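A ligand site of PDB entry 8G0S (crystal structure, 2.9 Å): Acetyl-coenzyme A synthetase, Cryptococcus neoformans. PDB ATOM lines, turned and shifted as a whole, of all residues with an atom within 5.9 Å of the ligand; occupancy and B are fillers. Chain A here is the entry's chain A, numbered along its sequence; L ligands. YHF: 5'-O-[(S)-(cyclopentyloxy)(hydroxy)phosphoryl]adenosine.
The side-chain carboxylate (OD2) of Asp 541 lies within hydrogen-bond range of an oxygen (O1) of the ligand (2.4 Å). The backbone carbonyl oxygen (O) of Thr 451 sits at hydrogen-bond distance from a nitrogen (N5) of the ligand (2.8 Å). N of Thr 455 is in hydrogen-bond range of O5 of the ligand (3.0 Å). An oxygen (O5) of the ligand lies within hydrogen-bond range of the side-chain hydroxyl of Thr 455. N of Gly 426 lies within hydrogen-bond range of N2 of the ligand (3.4 Å). SD of Met 454 sits at hydrogen-bond distance from O1 of the ligand. OD1 of Asp 450 is in hydrogen-bond range of N5 of the ligand.
OH of Tyr 452 is in hydrogen-bond range of OD2 of Asp 541, at 2.6 Å. O of Ser 424 is in hydrogen-bond range of N of Thr 451 (3.0 Å).
Ile 349 touches the ligand (CG2 to C15, 3.5 Å). OG1 of Thr 350 touches C15 of the ligand, at 3.2 Å. Val 425 touches the ligand. Glu 427 touches the ligand. Pro 428 touches the ligand. Tyr 452 touches the ligand (CA to N5, 3.7 Å). O of Trp 453 touches C13 of the ligand (3.3 Å). CG2 of Ile 553 touches C7 of the ligand (3.7 Å). CE of Lys 554 touches O3 of the ligand, 3.3 Å away. Hydrophobic or aromatic side chains within 4 Å of the ligand: Ile 349, Val 425, Pro 428, Tyr 452, Trp 453, Met 454 and Ile 553.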
ATOM      1  N   THR A 303       4.268  -1.028 -12.216  1.00  0.00           N
ATOM      2  CA  THR A 303       2.831  -0.916 -12.428  1.00  0.00           C
ATOM      3  C   THR A 303       2.524  -0.100 -13.685  1.00  0.00           C
ATOM      4  O   THR A 303       3.275   0.793 -14.074  1.00  0.00           O
ATOM      5  CB  THR A 303       2.166  -0.276 -11.215  1.00  0.00           C
ATOM      6  OG1 THR A 303       2.718   1.037 -11.022  1.00  0.00           O
ATOM      7  CG2 THR A 303       2.418  -1.122  -9.983  1.00  0.00           C
ATOM      8  N   TRP A 348       1.968  -9.348 -14.827  1.00  0.00           N
ATOM      9  CA  TRP A 348       1.308  -8.782 -13.659  1.00  0.00           C
ATOM     10  C   TRP A 348       1.666  -9.579 -12.404  1.00  0.00           C
ATOM     11  O   TRP A 348       2.143 -10.715 -12.488  1.00  0.00           O
ATOM     12  CB  TRP A 348      -0.213  -8.771 -13.859  1.00  0.00           C
ATOM     13  CG  TRP A 348      -0.633  -8.234 -15.215  1.00  0.00           C
ATOM     14  CD1 TRP A 348      -1.508  -8.822 -16.090  1.00  0.00           C
ATOM     15  CD2 TRP A 348      -0.203  -7.007 -15.828  1.00  0.00           C
ATOM     16  NE1 TRP A 348      -1.639  -8.047 -17.211  1.00  0.00           N
ATOM     17  CE2 TRP A 348      -0.853  -6.925 -17.084  1.00  0.00           C
ATOM     18  CE3 TRP A 348       0.659  -5.973 -15.451  1.00  0.00           C
ATOM     19  CZ2 TRP A 348      -0.667  -5.854 -17.949  1.00  0.00           C
ATOM     20  CZ3 TRP A 348       0.843  -4.915 -16.322  1.00  0.00           C
ATOM     21  CH2 TRP A 348       0.186  -4.855 -17.549  1.00  0.00           C
ATOM     22  N   ILE A 349       1.441  -8.956 -11.241  1.00  0.00           N
ATOM     23  CA  ILE A 349       1.783  -9.609  -9.985  1.00  0.00           C
ATOM     24  C   ILE A 349       0.993 -10.909  -9.806  1.00  0.00           C
ATOM     25  O   ILE A 349       1.452 -11.830  -9.116  1.00  0.00           O
ATOM     26  CB  ILE A 349       1.557  -8.644  -8.790  1.00  0.00           C
ATOM     27  CG1 ILE A 349       2.179  -9.197  -7.509  1.00  0.00           C
ATOM     28  CG2 ILE A 349       0.084  -8.414  -8.551  1.00  0.00           C
ATOM     29  CD1 ILE A 349       3.689  -9.175  -7.513  1.00  0.00           C
ATOM     30  N   THR A 350      -0.174 -11.011 -10.443  1.00  0.00           N
ATOM     31  CA  THR A 350      -0.939 -12.262 -10.351  1.00  0.00           C
ATOM     32  C   THR A 350      -0.166 -13.406 -10.972  1.00  0.00           C
ATOM     33  O   THR A 350      -0.114 -14.507 -10.399  1.00  0.00           O
ATOM     34  CB  THR A 350      -2.284 -12.111 -11.055  1.00  0.00           C
ATOM     35  OG1 THR A 350      -2.869 -10.847 -10.728  1.00  0.00           O
ATOM     36  CG2 THR A 350      -3.221 -13.229 -10.620  1.00  0.00           C
ATOM     37  N   SER A 424     -11.577 -15.361  -8.003  1.00  0.00           N
ATOM     38  CA  SER A 424     -11.761 -14.120  -8.743  1.00  0.00           C
ATOM     39  C   SER A 424     -10.805 -13.073  -8.192  1.00  0.00           C
ATOM     40  O   SER A 424     -10.647 -12.954  -6.971  1.00  0.00           O
ATOM     41  CB  SER A 424     -13.194 -13.639  -8.647  1.00  0.00           C
ATOM     42  OG  SER A 424     -13.290 -12.313  -9.119  1.00  0.00           O
ATOM     43  N   VAL A 425     -10.162 -12.308  -9.090  1.00  0.00           N
ATOM     44  CA  VAL A 425      -9.157 -11.320  -8.687  1.00  0.00           C
ATOM     45  C   VAL A 425      -9.153 -10.173  -9.691  1.00  0.00           C
ATOM     46  O   VAL A 425      -9.444 -10.357 -10.880  1.00  0.00           O
ATOM     47  CB  VAL A 425      -7.751 -11.938  -8.569  1.00  0.00           C
ATOM     48  CG1 VAL A 425      -7.265 -12.477  -9.909  1.00  0.00           C
ATOM     49  CG2 VAL A 425      -6.770 -10.917  -8.021  1.00  0.00           C
ATOM     50  N   GLY A 426      -8.841  -8.970  -9.210  1.00  0.00           N
ATOM     51  CA  GLY A 426      -8.573  -7.813 -10.043  1.00  0.00           C
ATOM     52  C   GLY A 426      -9.484  -6.628  -9.819  1.00  0.00           C
ATOM     53  O   GLY A 426      -9.051  -5.479  -9.948  1.00  0.00           O
ATOM     54  N   GLU A 427     -10.740  -6.864  -9.464  1.00  0.00           N
ATOM     55  CA  GLU A 427     -11.715  -5.794  -9.359  1.00  0.00           C
ATOM     56  C   GLU A 427     -12.947  -6.313  -8.610  1.00  0.00           C
ATOM     57  O   GLU A 427     -13.109  -7.522  -8.454  1.00  0.00           O
ATOM     58  CB  GLU A 427     -12.117  -5.274 -10.748  1.00  0.00           C
ATOM     59  CG  GLU A 427     -12.828  -6.300 -11.616  1.00  0.00           C
ATOM     60  CD  GLU A 427     -13.441  -5.685 -12.878  1.00  0.00           C
ATOM     61  OE1 GLU A 427     -13.083  -4.539 -13.222  1.00  0.00           O
ATOM     62  OE2 GLU A 427     -14.277  -6.351 -13.515  1.00  0.00           O
ATOM     63  N   PRO A 428     -13.808  -5.418  -8.109  1.00  0.00           N
ATOM     64  CA  PRO A 428     -15.035  -5.881  -7.456  1.00  0.00           C
ATOM     65  C   PRO A 428     -15.886  -6.674  -8.435  1.00  0.00           C
ATOM     66  O   PRO A 428     -15.990  -6.322  -9.607  1.00  0.00           O
ATOM     67  CB  PRO A 428     -15.732  -4.578  -7.024  1.00  0.00           C
ATOM     68  CG  PRO A 428     -14.665  -3.567  -6.993  1.00  0.00           C
ATOM     69  CD  PRO A 428     -13.716  -3.945  -8.079  1.00  0.00           C
ATOM     70  N   ILE A 429     -16.486  -7.752  -7.951  1.00  0.00           N
ATOM     71  CA  ILE A 429     -17.311  -8.621  -8.772  1.00  0.00           C
ATOM     72  C   ILE A 429     -18.779  -8.386  -8.418  1.00  0.00           C
ATOM     73  O   ILE A 429     -19.162  -8.457  -7.250  1.00  0.00           O
ATOM     74  CB  ILE A 429     -16.901 -10.096  -8.610  1.00  0.00           C
ATOM     75  CG1 ILE A 429     -17.800 -11.003  -9.464  1.00  0.00           C
ATOM     76  CG2 ILE A 429     -16.906 -10.521  -7.145  1.00  0.00           C
ATOM     77  CD1 ILE A 429     -17.258 -12.416  -9.613  1.00  0.00           C
ATOM     78  N   ASP A 450     -13.122 -14.773  -3.461  1.00  0.00           N
ATOM     79  CA  ASP A 450     -12.922 -13.405  -3.925  1.00  0.00           C
ATOM     80  C   ASP A 450     -11.682 -12.852  -3.234  1.00  0.00           C
ATOM     81  O   ASP A 450     -11.700 -12.597  -2.021  1.00  0.00           O
ATOM     82  CB  ASP A 450     -14.159 -12.562  -3.612  1.00  0.00           C
ATOM     83  CG  ASP A 450     -14.158 -11.238  -4.337  1.00  0.00           C
ATOM     84  OD1 ASP A 450     -13.227 -11.011  -5.134  1.00  0.00           O
ATOM     85  OD2 ASP A 450     -15.096 -10.438  -4.116  1.00  0.00           O
ATOM     86  N   THR A 451     -10.607 -12.687  -3.989  1.00  0.00           N
ATOM     87  CA  THR A 451      -9.324 -12.315  -3.424  1.00  0.00           C
ATOM     88  C   THR A 451      -9.053 -10.841  -3.688  1.00  0.00           C
ATOM     89  O   THR A 451      -9.079 -10.398  -4.836  1.00  0.00           O
ATOM     90  CB  THR A 451      -8.195 -13.164  -4.012  1.00  0.00           C
ATOM     91  OG1 THR A 451      -8.050 -12.900  -5.414  1.00  0.00           O
ATOM     92  CG2 THR A 451      -8.480 -14.651  -3.799  1.00  0.00           C
ATOM     93  N   TYR A 452      -8.795 -10.091  -2.615  1.00  0.00           N
ATOM     94  CA  TYR A 452      -8.369  -8.695  -2.714  1.00  0.00           C
ATOM     95  C   TYR A 452      -6.910  -8.609  -2.314  1.00  0.00           C
ATOM     96  O   TYR A 452      -6.517  -9.107  -1.249  1.00  0.00           O
ATOM     97  CB  TYR A 452      -9.227  -7.791  -1.806  1.00  0.00           C
ATOM     98  CG  TYR A 452      -8.613  -6.413  -1.597  1.00  0.00           C
ATOM     99  CD1 TYR A 452      -8.783  -5.405  -2.539  1.00  0.00           C
ATOM    100  CD2 TYR A 452      -7.859  -6.125  -0.463  1.00  0.00           C
ATOM    101  CE1 TYR A 452      -8.217  -4.149  -2.361  1.00  0.00           C
ATOM    102  CE2 TYR A 452      -7.301  -4.875  -0.272  1.00  0.00           C
ATOM    103  CZ  TYR A 452      -7.491  -3.889  -1.229  1.00  0.00           C
ATOM    104  OH  TYR A 452      -6.928  -2.644  -1.044  1.00  0.00           O
ATOM    105  N   TRP A 453      -6.106  -7.966  -3.149  1.00  0.00           N
ATOM    106  CA  TRP A 453      -4.711  -7.656  -2.816  1.00  0.00           C
ATOM    107  C   TRP A 453      -4.200  -6.679  -3.865  1.00  0.00           C
ATOM    108  O   TRP A 453      -4.955  -6.221  -4.740  1.00  0.00           O
ATOM    109  CB  TRP A 453      -3.846  -8.920  -2.733  1.00  0.00           C
ATOM    110  CG  TRP A 453      -3.804  -9.755  -3.972  1.00  0.00           C
ATOM    111  CD1 TRP A 453      -4.862 -10.322  -4.626  1.00  0.00           C
ATOM    112  CD2 TRP A 453      -2.633 -10.158  -4.696  1.00  0.00           C
ATOM    113  NE1 TRP A 453      -4.424 -11.022  -5.717  1.00  0.00           N
ATOM    114  CE2 TRP A 453      -3.055 -10.940  -5.777  1.00  0.00           C
ATOM    115  CE3 TRP A 453      -1.261  -9.931  -4.523  1.00  0.00           C
ATOM    116  CZ2 TRP A 453      -2.169 -11.489  -6.700  1.00  0.00           C
ATOM    117  CZ3 TRP A 453      -0.380 -10.474  -5.440  1.00  0.00           C
ATOM    118  CH2 TRP A 453      -0.827 -11.247  -6.503  1.00  0.00           C
ATOM    119  N   MET A 454      -2.929  -6.334  -3.762  1.00  0.00           N
ATOM    120  CA  MET A 454      -2.313  -5.355  -4.650  1.00  0.00           C
ATOM    121  C   MET A 454      -0.908  -5.811  -5.009  1.00  0.00           C
ATOM    122  O   MET A 454      -0.343  -6.709  -4.373  1.00  0.00           O
ATOM    123  CB  MET A 454      -2.260  -3.967  -4.005  1.00  0.00           C
ATOM    124  CG  MET A 454      -3.569  -3.400  -3.558  1.00  0.00           C
ATOM    125  SD  MET A 454      -3.362  -1.710  -2.961  1.00  0.00           S
ATOM    126  CE  MET A 454      -2.012  -1.914  -1.810  1.00  0.00           C
ATOM    127  N   THR A 455      -0.323  -5.153  -6.012  1.00  0.00           N
ATOM    128  CA  THR A 455       1.079  -5.408  -6.343  1.00  0.00           C
ATOM    129  C   THR A 455       1.965  -5.157  -5.135  1.00  0.00           C
ATOM    130  O   THR A 455       2.945  -5.874  -4.915  1.00  0.00           O
ATOM    131  CB  THR A 455       1.518  -4.537  -7.528  1.00  0.00           C
ATOM    132  OG1 THR A 455       0.604  -4.694  -8.617  1.00  0.00           O
ATOM    133  CG2 THR A 455       2.902  -4.954  -7.991  1.00  0.00           C
ATOM    134  N   GLU A 456       1.625  -4.146  -4.334  1.00  0.00           N
ATOM    135  CA  GLU A 456       2.447  -3.800  -3.190  1.00  0.00           C
ATOM    136  C   GLU A 456       2.265  -4.760  -2.013  1.00  0.00           C
ATOM    137  O   GLU A 456       3.113  -4.772  -1.110  1.00  0.00           O
ATOM    138  CB  GLU A 456       2.122  -2.377  -2.732  1.00  0.00           C
ATOM    139  CG  GLU A 456       2.252  -1.312  -3.824  1.00  0.00           C
ATOM    140  CD  GLU A 456       0.983  -1.174  -4.675  1.00  0.00           C
ATOM    141  OE1 GLU A 456       0.150  -2.097  -4.665  1.00  0.00           O
ATOM    142  OE2 GLU A 456       0.815  -0.123  -5.342  1.00  0.00           O
ATOM    143  N   ALA A 476     -15.030  -9.836  -0.151  1.00  0.00           N
ATOM    144  CA  ALA A 476     -13.740 -10.483   0.049  1.00  0.00           C
ATOM    145  C   ALA A 476     -13.638 -11.182   1.403  1.00  0.00           C
ATOM    146  O   ALA A 476     -12.624 -11.849   1.659  1.00  0.00           O
ATOM    147  CB  ALA A 476     -12.603  -9.465  -0.092  1.00  0.00           C
ATOM    148  N   PHE A 539      -3.942   1.237   1.837  1.00  0.00           N
ATOM    149  CA  PHE A 539      -4.208   0.545   0.574  1.00  0.00           C
ATOM    150  C   PHE A 539      -4.669   1.499  -0.526  1.00  0.00           C
ATOM    151  O   PHE A 539      -4.451   1.225  -1.715  1.00  0.00           O
ATOM    152  CB  PHE A 539      -5.279  -0.541   0.755  1.00  0.00           C
ATOM    153  CG  PHE A 539      -4.822  -1.721   1.564  1.00  0.00           C
ATOM    154  CD1 PHE A 539      -4.972  -1.723   2.953  1.00  0.00           C
ATOM    155  CD2 PHE A 539      -4.275  -2.835   0.951  1.00  0.00           C
ATOM    156  CE1 PHE A 539      -4.574  -2.812   3.706  1.00  0.00           C
ATOM    157  CE2 PHE A 539      -3.865  -3.935   1.692  1.00  0.00           C
ATOM    158  CZ  PHE A 539      -4.013  -3.925   3.073  1.00  0.00           C
ATOM    159  N   GLY A 540      -5.345   2.582  -0.153  1.00  0.00           N
ATOM    160  CA  GLY A 540      -5.917   3.500  -1.127  1.00  0.00           C
ATOM    161  C   GLY A 540      -7.282   3.109  -1.636  1.00  0.00           C
ATOM    162  O   GLY A 540      -7.773   3.730  -2.593  1.00  0.00           O
ATOM    163  N   ASP A 541      -7.918   2.106  -1.041  1.00  0.00           N
ATOM    164  CA  ASP A 541      -9.244   1.671  -1.443  1.00  0.00           C
ATOM    165  C   ASP A 541     -10.195   1.891  -0.282  1.00  0.00           C
ATOM    166  O   ASP A 541      -9.840   1.684   0.879  1.00  0.00           O
ATOM    167  CB  ASP A 541      -9.258   0.191  -1.821  1.00  0.00           C
ATOM    168  CG  ASP A 541      -8.411  -0.108  -3.024  1.00  0.00           C
ATOM    169  OD1 ASP A 541      -8.567   0.589  -4.049  1.00  0.00           O
ATOM    170  OD2 ASP A 541      -7.589  -1.044  -2.934  1.00  0.00           O
ATOM    171  N   ILE A 553     -14.854  -4.511  -0.303  1.00  0.00           N
ATOM    172  CA  ILE A 553     -13.920  -3.554  -0.889  1.00  0.00           C
ATOM    173  C   ILE A 553     -14.661  -2.746  -1.938  1.00  0.00           C
ATOM    174  O   ILE A 553     -15.482  -3.280  -2.697  1.00  0.00           O
ATOM    175  CB  ILE A 553     -12.713  -4.298  -1.484  1.00  0.00           C
ATOM    176  CG1 ILE A 553     -12.143  -5.314  -0.489  1.00  0.00           C
ATOM    177  CG2 ILE A 553     -11.636  -3.321  -1.906  1.00  0.00           C
ATOM    178  CD1 ILE A 553     -11.470  -4.692   0.725  1.00  0.00           C
ATOM    179  N   LYS A 554     -14.415  -1.429  -1.951  1.00  0.00           N
ATOM    180  CA  LYS A 554     -15.054  -0.474  -2.856  1.00  0.00           C
ATOM    181  C   LYS A 554     -16.552  -0.347  -2.598  1.00  0.00           C
ATOM    182  O   LYS A 554     -17.228   0.409  -3.307  1.00  0.00           O
ATOM    183  CB  LYS A 554     -14.841  -0.816  -4.334  1.00  0.00           C
ATOM    184  CG  LYS A 554     -13.852   0.063  -5.094  1.00  0.00           C
ATOM    185  CD  LYS A 554     -12.408  -0.343  -4.838  1.00  0.00           C
ATOM    186  CE  LYS A 554     -11.513   0.050  -6.001  1.00  0.00           C
ATOM    187  NZ  LYS A 554     -11.755  -0.781  -7.230  1.00  0.00           N
HETATM  188  C1  YHF L   1      -6.736  -2.661  -5.530  1.00  0.00           C
HETATM  189  C10 YHF L   1      -4.889  -3.618  -7.057  1.00  0.00           C
HETATM  190  C11 YHF L   1      -3.841  -6.512  -9.331  1.00  0.00           C
HETATM  191  C12 YHF L   1      -5.030  -6.935  -8.498  1.00  0.00           C
HETATM  192  C13 YHF L   1      -4.378  -7.879  -7.492  1.00  0.00           C
HETATM  193  C14 YHF L   1      -3.522  -8.711  -8.383  1.00  0.00           C
HETATM  194  C15 YHF L   1      -3.194  -7.856  -9.608  1.00  0.00           C
HETATM  195  C2  YHF L   1      -8.202  -2.358  -5.845  1.00  0.00           C
HETATM  196  C3  YHF L   1      -8.434  -3.301  -7.028  1.00  0.00           C
HETATM  197  C4  YHF L   1      -8.060  -5.823  -6.886  1.00  0.00           C
HETATM  198  C5  YHF L   1      -9.884  -6.475  -5.979  1.00  0.00           C
HETATM  199  C6  YHF L   1      -9.980  -5.104  -6.098  1.00  0.00           C
HETATM  200  C7  YHF L   1     -11.986  -5.058  -5.206  1.00  0.00           C
HETATM  201  C8  YHF L   1     -10.989  -7.143  -5.405  1.00  0.00           C
HETATM  202  C9  YHF L   1      -6.144  -2.791  -6.945  1.00  0.00           C
HETATM  203  N1  YHF L   1      -8.804  -4.678  -6.683  1.00  0.00           N
HETATM  204  N2  YHF L   1      -8.679  -6.921  -6.468  1.00  0.00           N
HETATM  205  N3  YHF L   1     -11.009  -4.318  -5.736  1.00  0.00           N
HETATM  206  N4  YHF L   1     -12.050  -6.383  -5.016  1.00  0.00           N
HETATM  207  N5  YHF L   1     -11.046  -8.461  -5.214  1.00  0.00           N
HETATM  208  O1  YHF L   1      -6.098  -1.656  -4.762  1.00  0.00           O
HETATM  209  O2  YHF L   1      -7.197  -3.359  -7.742  1.00  0.00           O
HETATM  210  O3  YHF L   1      -8.378  -1.010  -6.264  1.00  0.00           O
HETATM  211  O4  YHF L   1      -4.434  -3.625  -8.433  1.00  0.00           O
HETATM  212  O5  YHF L   1      -2.030  -3.438  -7.785  1.00  0.00           O
HETATM  213  O6  YHF L   1      -2.970  -5.688  -8.559  1.00  0.00           O
HETATM  214  O7  YHF L   1      -2.726  -3.818 -10.225  1.00  0.00           O
HETATM  215  P1  YHF L   1      -2.940  -4.100  -8.773  1.00  0.00           P
